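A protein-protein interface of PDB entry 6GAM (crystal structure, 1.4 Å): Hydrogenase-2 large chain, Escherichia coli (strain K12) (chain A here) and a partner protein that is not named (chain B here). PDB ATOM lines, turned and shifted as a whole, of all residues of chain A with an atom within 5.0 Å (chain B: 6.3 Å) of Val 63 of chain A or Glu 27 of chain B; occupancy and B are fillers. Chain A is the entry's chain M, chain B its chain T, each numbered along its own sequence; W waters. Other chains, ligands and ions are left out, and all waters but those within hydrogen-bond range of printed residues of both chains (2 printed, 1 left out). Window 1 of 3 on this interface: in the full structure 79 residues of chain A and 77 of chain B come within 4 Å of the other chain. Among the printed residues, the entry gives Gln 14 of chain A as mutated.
The backbone NH (N) of Gly 62 of chain A is in hydrogen-bond range of the backbone carbonyl oxygen (O) of Cys 22 of chain B (2.8 Å).
The side-chain amide nitrogen of Gln 14 of chain A lies within hydrogen-bond range of the side-chain hydroxyl of Thr 23 of chain B (2.7 Å).
OE1 of Gln 14 of chain A sits close to SG of Cys 546 of chain A, at 3.5 Å.
The side-chain carboxylate (OE1) of Glu 27 of chain B is in salt-bridge range of the guanidinium group (NH1) of Arg 31 of chain B, at 2.9 Å.
The backbone NH of Gly 24 of chain B sits close to the side-chain sulfur of Cys 22 of chain B (3.3 Å).
OG of Ser 28 of chain B is in hydrogen-bond range of O of Cys 25 of chain B.
The side-chain sulfur (SG) of Cys 61 of chain A sits close to the backbone NH (N) of Val 63 of chain A (3.5 Å).
NE2 of His 99 of chain A sits close to O of Val 63 of chain A.
Gln 14 of chain A touches Cys 22 of chain B.
Gly 62 of chain A touches Gly 24 of chain B (CA to N, 3.7 Å).
Val 63 of chain A touches Glu 27 of chain B.
OE1 of Glu 27 of chain B touches CE1 of His 102 of chain A, at 3.4 Å.
His 102 of chain A touches Arg 31 of chain B.
CG of Pro 213 of chain A touches O of Gly 24 of chain B, 3.5 Å away.
Glu 27 of chain B touches Pro 213 of chain A (CB to CG, 3.7 Å).
Pro 213 of chain A touches Ser 28 of chain B.
Arg 31 of chain B touches Pro 213 of chain A (NE to CD, 3.4 Å).
Pro 213 of chain A touches Pro 155 of chain B (O to CD, 3.4 Å).
Val 63 of chain A touches just these residues of chain B: Cys 22, Thr 23 and Glu 27.
Glu 27 of chain B touches four residues of chain A.
Printed residues of chain B within 4 Å of His 102 of chain A: Glu 27 (3.4 Å) and Arg 31 (3.6 Å).
Of the printed residues of chain B, Gly 62 of chain A touches Cys 22, Gly 24 and Glu 27.
Of the printed residues of chain A, Arg 31 of chain B touches His 102 and Pro 213.
Of the printed residues of chain B, Cys 61 of chain A touches Cys 22 (3.8 Å).
Of the printed residues of chain A, Ser 28 of chain B touches Pro 213 (3.8 Å).
The nearest printed residue of chain A that does not touch Glu 27 of chain B is Cys 64 of chain A (6.0 Å).
The nearest printed residue of chain B that does not touch Cys 61 of chain A is Gly 24 of chain B (5.5 Å).
Hydrophobic or aromatic side chains of chain A that line the printed part of chain B: Val 63, His 102 and Pro 213.
Among the printed residues, 16 pairs touch across the chains.
Water W1 bridges the side-chain carboxylate of Glu 27 of chain B (2.6 Å) and a ring nitrogen (NE2) of His 102 of chain A (3.0 Å).
Water W2 lies within hydrogen-bond range of ND1 of His 99 of chain A (2.9 Å) and NH2 of Arg 31 of chain B (3.5 Å).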
ATOM      1  N   GLN A  14       4.267  20.512  24.910  1.00  0.00           N
ATOM      2  CA  GLN A  14       5.208  20.315  26.014  1.00  0.00           C
ATOM      3  C   GLN A  14       4.410  20.082  27.295  1.00  0.00           C
ATOM      4  O   GLN A  14       3.532  20.914  27.629  1.00  0.00           O
ATOM      5  CB  GLN A  14       6.167  21.510  26.162  1.00  0.00           C
ATOM      6  CG  GLN A  14       7.309  21.223  27.108  1.00  0.00           C
ATOM      7  CD  GLN A  14       6.909  21.033  28.541  1.00  0.00           C
ATOM      8  OE1 GLN A  14       5.978  21.737  29.020  1.00  0.00           O
ATOM      9  NE2 GLN A  14       7.572  20.112  29.269  1.00  0.00           N
ATOM     10  N   CYS A  61      11.980  25.186  31.048  1.00  0.00           N
ATOM     11  CA  CYS A  61      11.521  24.546  29.817  1.00  0.00           C
ATOM     12  C   CYS A  61      12.641  24.313  28.836  1.00  0.00           C
ATOM     13  O   CYS A  61      13.445  25.225  28.600  1.00  0.00           O
ATOM     14  CB  CYS A  61      10.453  25.376  29.158  1.00  0.00           C
ATOM     15  SG  CYS A  61       9.635  24.587  27.762  1.00  0.00           S
ATOM     16  N   GLY A  62      12.662  23.118  28.252  1.00  0.00           N
ATOM     17  CA  GLY A  62      13.628  22.770  27.210  1.00  0.00           C
ATOM     18  C   GLY A  62      13.093  22.858  25.803  1.00  0.00           C
ATOM     19  O   GLY A  62      13.875  22.755  24.845  1.00  0.00           O
ATOM     20  N   VAL A  63      11.782  22.966  25.594  1.00  0.00           N
ATOM     21  CA  VAL A  63      11.244  23.292  24.307  1.00  0.00           C
ATOM     22  C   VAL A  63      11.525  24.759  24.039  1.00  0.00           C
ATOM     23  O   VAL A  63      12.252  25.063  23.094  1.00  0.00           O
ATOM     24  CB  VAL A  63       9.744  22.980  24.244  1.00  0.00           C
ATOM     25  CG1 VAL A  63       9.136  23.458  22.945  1.00  0.00           C
ATOM     26  CG2 VAL A  63       9.527  21.473  24.430  1.00  0.00           C
ATOM     27  N   CYS A  64      11.034  25.666  24.877  1.00  0.00           N
ATOM     28  CA  CYS A  64      11.459  27.075  24.801  1.00  0.00           C
ATOM     29  C   CYS A  64      12.711  27.320  25.600  1.00  0.00           C
ATOM     30  O   CYS A  64      12.822  28.244  26.428  1.00  0.00           O
ATOM     31  CB  CYS A  64      10.322  28.020  25.156  1.00  0.00           C
ATOM     32  SG  CYS A  64       9.709  27.876  26.860  1.00  0.00           S
ATOM     33  N   THR A  65      13.725  26.490  25.325  1.00  0.00           N
ATOM     34  CA  THR A  65      15.049  26.763  25.855  1.00  0.00           C
ATOM     35  C   THR A  65      15.486  28.115  25.320  1.00  0.00           C
ATOM     36  O   THR A  65      14.877  28.667  24.392  1.00  0.00           O
ATOM     37  CB  THR A  65      15.994  25.593  25.498  1.00  0.00           C
ATOM     38  OG1 THR A  65      17.230  25.784  26.180  1.00  0.00           O
ATOM     39  CG2 THR A  65      16.233  25.495  24.040  1.00  0.00           C
ATOM     40  N   HIS A  99      16.361  30.207  17.708  1.00  0.00           N
ATOM     41  CA  HIS A  99      15.629  29.275  18.548  1.00  0.00           C
ATOM     42  C   HIS A  99      14.160  29.274  18.134  1.00  0.00           C
ATOM     43  O   HIS A  99      13.569  28.197  17.916  1.00  0.00           O
ATOM     44  CB  HIS A  99      15.708  29.601  20.045  1.00  0.00           C
ATOM     45  CG  HIS A  99      14.743  28.768  20.780  1.00  0.00           C
ATOM     46  ND1 HIS A  99      15.028  27.453  21.047  1.00  0.00           N
ATOM     47  CD2 HIS A  99      13.422  28.939  21.039  1.00  0.00           C
ATOM     48  CE1 HIS A  99      13.926  26.854  21.481  1.00  0.00           C
ATOM     49  NE2 HIS A  99      12.943  27.736  21.479  1.00  0.00           N
ATOM     50  N   HIS A 102      13.340  27.313  14.964  1.00  0.00           N
ATOM     51  CA  HIS A 102      13.212  25.887  15.278  1.00  0.00           C
ATOM     52  C   HIS A 102      11.874  25.597  15.959  1.00  0.00           C
ATOM     53  O   HIS A 102      11.203  24.612  15.634  1.00  0.00           O
ATOM     54  CB  HIS A 102      14.424  25.423  16.128  1.00  0.00           C
ATOM     55  CG  HIS A 102      14.086  24.424  17.195  1.00  0.00           C
ATOM     56  ND1 HIS A 102      14.045  23.054  16.999  1.00  0.00           N
ATOM     57  CD2 HIS A 102      13.747  24.634  18.484  1.00  0.00           C
ATOM     58  CE1 HIS A 102      13.702  22.484  18.141  1.00  0.00           C
ATOM     59  NE2 HIS A 102      13.494  23.406  19.054  1.00  0.00           N
ATOM     60  N   ASP A 103      11.538  26.398  16.920  1.00  0.00           N
ATOM     61  CA  ASP A 103      10.403  26.134  17.817  1.00  0.00           C
ATOM     62  C   ASP A 103       9.108  26.155  16.982  1.00  0.00           C
ATOM     63  O   ASP A 103       8.334  25.179  17.014  1.00  0.00           O
ATOM     64  CB  ASP A 103      10.431  27.190  18.926  1.00  0.00           C
ATOM     65  CG  ASP A 103       9.643  26.796  20.158  1.00  0.00           C
ATOM     66  OD1 ASP A 103       8.604  26.109  20.013  1.00  0.00           O
ATOM     67  OD2 ASP A 103      10.019  27.179  21.299  1.00  0.00           O
ATOM     68  N   PRO A 213      19.785  21.757  23.464  1.00  0.00           N
ATOM     69  CA  PRO A 213      19.111  22.609  24.463  1.00  0.00           C
ATOM     70  C   PRO A 213      19.982  23.125  25.578  1.00  0.00           C
ATOM     71  O   PRO A 213      21.009  22.513  25.915  1.00  0.00           O
ATOM     72  CB  PRO A 213      18.020  21.683  25.041  1.00  0.00           C
ATOM     73  CG  PRO A 213      17.845  20.592  24.016  1.00  0.00           C
ATOM     74  CD  PRO A 213      19.214  20.389  23.445  1.00  0.00           C
ATOM     75  N   ARG A 479       5.794  31.563  22.509  1.00  0.00           N
ATOM     76  CA  ARG A 479       4.393  31.410  22.929  1.00  0.00           C
ATOM     77  C   ARG A 479       3.805  32.669  23.504  1.00  0.00           C
ATOM     78  O   ARG A 479       2.633  32.680  23.869  1.00  0.00           O
ATOM     79  CB  ARG A 479       4.297  30.235  23.892  1.00  0.00           C
ATOM     80  CG  ARG A 479       4.526  28.871  23.216  1.00  0.00           C
ATOM     81  CD  ARG A 479       4.882  27.724  24.158  1.00  0.00           C
ATOM     82  NE  ARG A 479       5.238  26.572  23.328  1.00  0.00           N
ATOM     83  CZ  ARG A 479       6.392  26.406  22.679  1.00  0.00           C
ATOM     84  NH1 ARG A 479       7.403  27.229  22.880  1.00  0.00           N
ATOM     85  NH2 ARG A 479       6.527  25.390  21.827  1.00  0.00           N
ATOM     86  N   CYS A 546       2.622  24.925  26.548  1.00  0.00           N
ATOM     87  CA  CYS A 546       3.840  24.479  27.222  1.00  0.00           C
ATOM     88  C   CYS A 546       3.571  24.511  28.693  1.00  0.00           C
ATOM     89  O   CYS A 546       3.501  25.573  29.315  1.00  0.00           O
ATOM     90  CB  CYS A 546       4.975  25.399  26.861  1.00  0.00           C
ATOM     91  SG  CYS A 546       6.577  24.813  27.472  1.00  0.00           S
ATOM     92  N   CYS B  22      11.476  18.892  31.694  1.00  0.00           N
ATOM     93  CA  CYS B  22      11.367  20.161  30.994  1.00  0.00           C
ATOM     94  C   CYS B  22      11.277  19.953  29.477  1.00  0.00           C
ATOM     95  O   CYS B  22      11.025  20.901  28.728  1.00  0.00           O
ATOM     96  CB  CYS B  22      12.528  21.094  31.332  1.00  0.00           C
ATOM     97  SG  CYS B  22      14.046  20.734  30.381  1.00  0.00           S
ATOM     98  N   THR B  23      11.460  18.707  29.017  1.00  0.00           N
ATOM     99  CA  THR B  23      11.431  18.265  27.624  1.00  0.00           C
ATOM    100  C   THR B  23      12.771  18.467  26.912  1.00  0.00           C
ATOM    101  O   THR B  23      12.961  18.007  25.789  1.00  0.00           O
ATOM    102  CB  THR B  23      10.218  18.806  26.828  1.00  0.00           C
ATOM    103  OG1 THR B  23       9.040  18.540  27.620  1.00  0.00           O
ATOM    104  CG2 THR B  23      10.013  18.113  25.497  1.00  0.00           C
ATOM    105  N   GLY B  24      13.738  19.103  27.584  1.00  0.00           N
ATOM    106  CA  GLY B  24      15.058  19.243  26.994  1.00  0.00           C
ATOM    107  C   GLY B  24      15.718  17.933  26.617  1.00  0.00           C
ATOM    108  O   GLY B  24      16.448  17.872  25.623  1.00  0.00           O
ATOM    109  N   CYS B  25      15.436  16.864  27.356  1.00  0.00           N
ATOM    110  CA  CYS B  25      16.041  15.576  27.030  1.00  0.00           C
ATOM    111  C   CYS B  25      15.460  14.962  25.771  1.00  0.00           C
ATOM    112  O   CYS B  25      16.190  14.436  24.929  1.00  0.00           O
ATOM    113  CB  CYS B  25      15.935  14.626  28.253  1.00  0.00           C
ATOM    114  SG  CYS B  25      17.013  15.086  29.645  1.00  0.00           S
ATOM    115  N   THR B  26      14.142  15.043  25.564  1.00  0.00           N
ATOM    116  CA  THR B  26      13.569  14.711  24.250  1.00  0.00           C
ATOM    117  C   THR B  26      14.080  15.645  23.163  1.00  0.00           C
ATOM    118  O   THR B  26      14.442  15.201  22.049  1.00  0.00           O
ATOM    119  CB  THR B  26      12.051  14.797  24.307  1.00  0.00           C
ATOM    120  OG1 THR B  26      11.591  13.708  25.139  1.00  0.00           O
ATOM    121  CG2 THR B  26      11.495  14.722  22.972  1.00  0.00           C
ATOM    122  N   GLU B  27      14.120  16.954  23.463  1.00  0.00           N
ATOM    123  CA  GLU B  27      14.589  17.916  22.451  1.00  0.00           C
ATOM    124  C   GLU B  27      16.024  17.664  21.992  1.00  0.00           C
ATOM    125  O   GLU B  27      16.359  17.952  20.811  1.00  0.00           O
ATOM    126  CB  GLU B  27      14.484  19.325  23.027  1.00  0.00           C
ATOM    127  CG  GLU B  27      13.058  19.860  23.003  1.00  0.00           C
ATOM    128  CD  GLU B  27      12.577  20.288  21.645  1.00  0.00           C
ATOM    129  OE1 GLU B  27      13.270  20.209  20.626  1.00  0.00           O
ATOM    130  OE2 GLU B  27      11.376  20.723  21.562  1.00  0.00           O
ATOM    131  N   SER B  28      16.838  17.082  22.865  1.00  0.00           N
ATOM    132  CA  SER B  28      18.218  16.732  22.414  1.00  0.00           C
ATOM    133  C   SER B  28      18.157  15.838  21.169  1.00  0.00           C
ATOM    134  O   SER B  28      18.988  15.950  20.252  1.00  0.00           O
ATOM    135  CB  SER B  28      19.019  16.069  23.510  1.00  0.00           C
ATOM    136  OG  SER B  28      18.649  14.711  23.736  1.00  0.00           O
ATOM    137  N   LEU B  29      17.153  14.971  21.086  1.00  0.00           N
ATOM    138  CA  LEU B  29      17.039  14.104  19.912  1.00  0.00           C
ATOM    139  C   LEU B  29      16.879  14.818  18.596  1.00  0.00           C
ATOM    140  O   LEU B  29      17.264  14.310  17.556  1.00  0.00           O
ATOM    141  CB  LEU B  29      15.875  13.107  20.059  1.00  0.00           C
ATOM    142  CG  LEU B  29      15.905  12.249  21.328  1.00  0.00           C
ATOM    143  CD1 LEU B  29      14.658  11.358  21.350  1.00  0.00           C
ATOM    144  CD2 LEU B  29      17.162  11.374  21.416  1.00  0.00           C
ATOM    145  N   LEU B  30      16.275  16.005  18.648  1.00  0.00           N
ATOM    146  CA  LEU B  30      16.052  16.809  17.475  1.00  0.00           C
ATOM    147  C   LEU B  30      17.329  17.492  16.945  1.00  0.00           C
ATOM    148  O   LEU B  30      17.310  17.974  15.834  1.00  0.00           O
ATOM    149  CB  LEU B  30      14.930  17.873  17.681  1.00  0.00           C
ATOM    150  CG  LEU B  30      13.512  17.361  17.361  1.00  0.00           C
ATOM    151  CD1 LEU B  30      13.136  16.230  18.292  1.00  0.00           C
ATOM    152  CD2 LEU B  30      12.533  18.499  17.495  1.00  0.00           C
ATOM    153  N   ARG B  31      18.421  17.432  17.709  1.00  0.00           N
ATOM    154  CA  ARG B  31      19.745  17.854  17.269  1.00  0.00           C
ATOM    155  C   ARG B  31      20.587  16.701  16.779  1.00  0.00           C
ATOM    156  O   ARG B  31      21.620  16.920  16.134  1.00  0.00           O
ATOM    157  CB  ARG B  31      20.493  18.567  18.403  1.00  0.00           C
ATOM    158  CG  ARG B  31      19.991  19.962  18.808  1.00  0.00           C
ATOM    159  CD  ARG B  31      18.655  19.910  19.520  1.00  0.00           C
ATOM    160  NE  ARG B  31      18.367  21.188  20.203  1.00  0.00           N
ATOM    161  CZ  ARG B  31      17.162  21.611  20.497  1.00  0.00           C
ATOM    162  NH1 ARG B  31      16.100  20.839  20.240  1.00  0.00           N
ATOM    163  NH2 ARG B  31      16.981  22.776  21.119  1.00  0.00           N
ATOM    164  N   ALA B  32      20.179  15.474  17.056  1.00  0.00           N
ATOM    165  CA  ALA B  32      20.990  14.318  16.751  1.00  0.00           C
ATOM    166  C   ALA B  32      21.156  14.130  15.228  1.00  0.00           C
ATOM    167  O   ALA B  32      20.274  14.492  14.450  1.00  0.00           O
ATOM    168  CB  ALA B  32      20.391  13.046  17.353  1.00  0.00           C
ATOM    169  N   VAL B  52       5.282  13.535  23.417  1.00  0.00           N
ATOM    170  CA  VAL B  52       5.581  14.717  22.645  1.00  0.00           C
ATOM    171  C   VAL B  52       5.216  14.546  21.192  1.00  0.00           C
ATOM    172  O   VAL B  52       4.813  15.494  20.541  1.00  0.00           O
ATOM    173  CB  VAL B  52       7.071  15.124  22.797  1.00  0.00           C
ATOM    174  CG1 VAL B  52       7.422  16.290  21.879  1.00  0.00           C
ATOM    175  CG2 VAL B  52       7.374  15.520  24.232  1.00  0.00           C
ATOM    176  N   PRO B 155      20.574  18.988  28.922  1.00  0.00           N
ATOM    177  CA  PRO B 155      20.492  17.537  28.692  1.00  0.00           C
ATOM    178  C   PRO B 155      21.827  16.990  28.189  1.00  0.00           C
ATOM    179  O   PRO B 155      22.683  17.752  27.714  1.00  0.00           O
ATOM    180  CB  PRO B 155      19.479  17.447  27.574  1.00  0.00           C
ATOM    181  CG  PRO B 155      19.734  18.691  26.740  1.00  0.00           C
ATOM    182  CD  PRO B 155      20.124  19.754  27.740  1.00  0.00           C
HETATM  183  O   HOH W   1      10.752  22.157  19.521  1.00  0.00           O
HETATM  184  O   HOH W   2      17.574  26.189  20.712  1.00  0.00           O
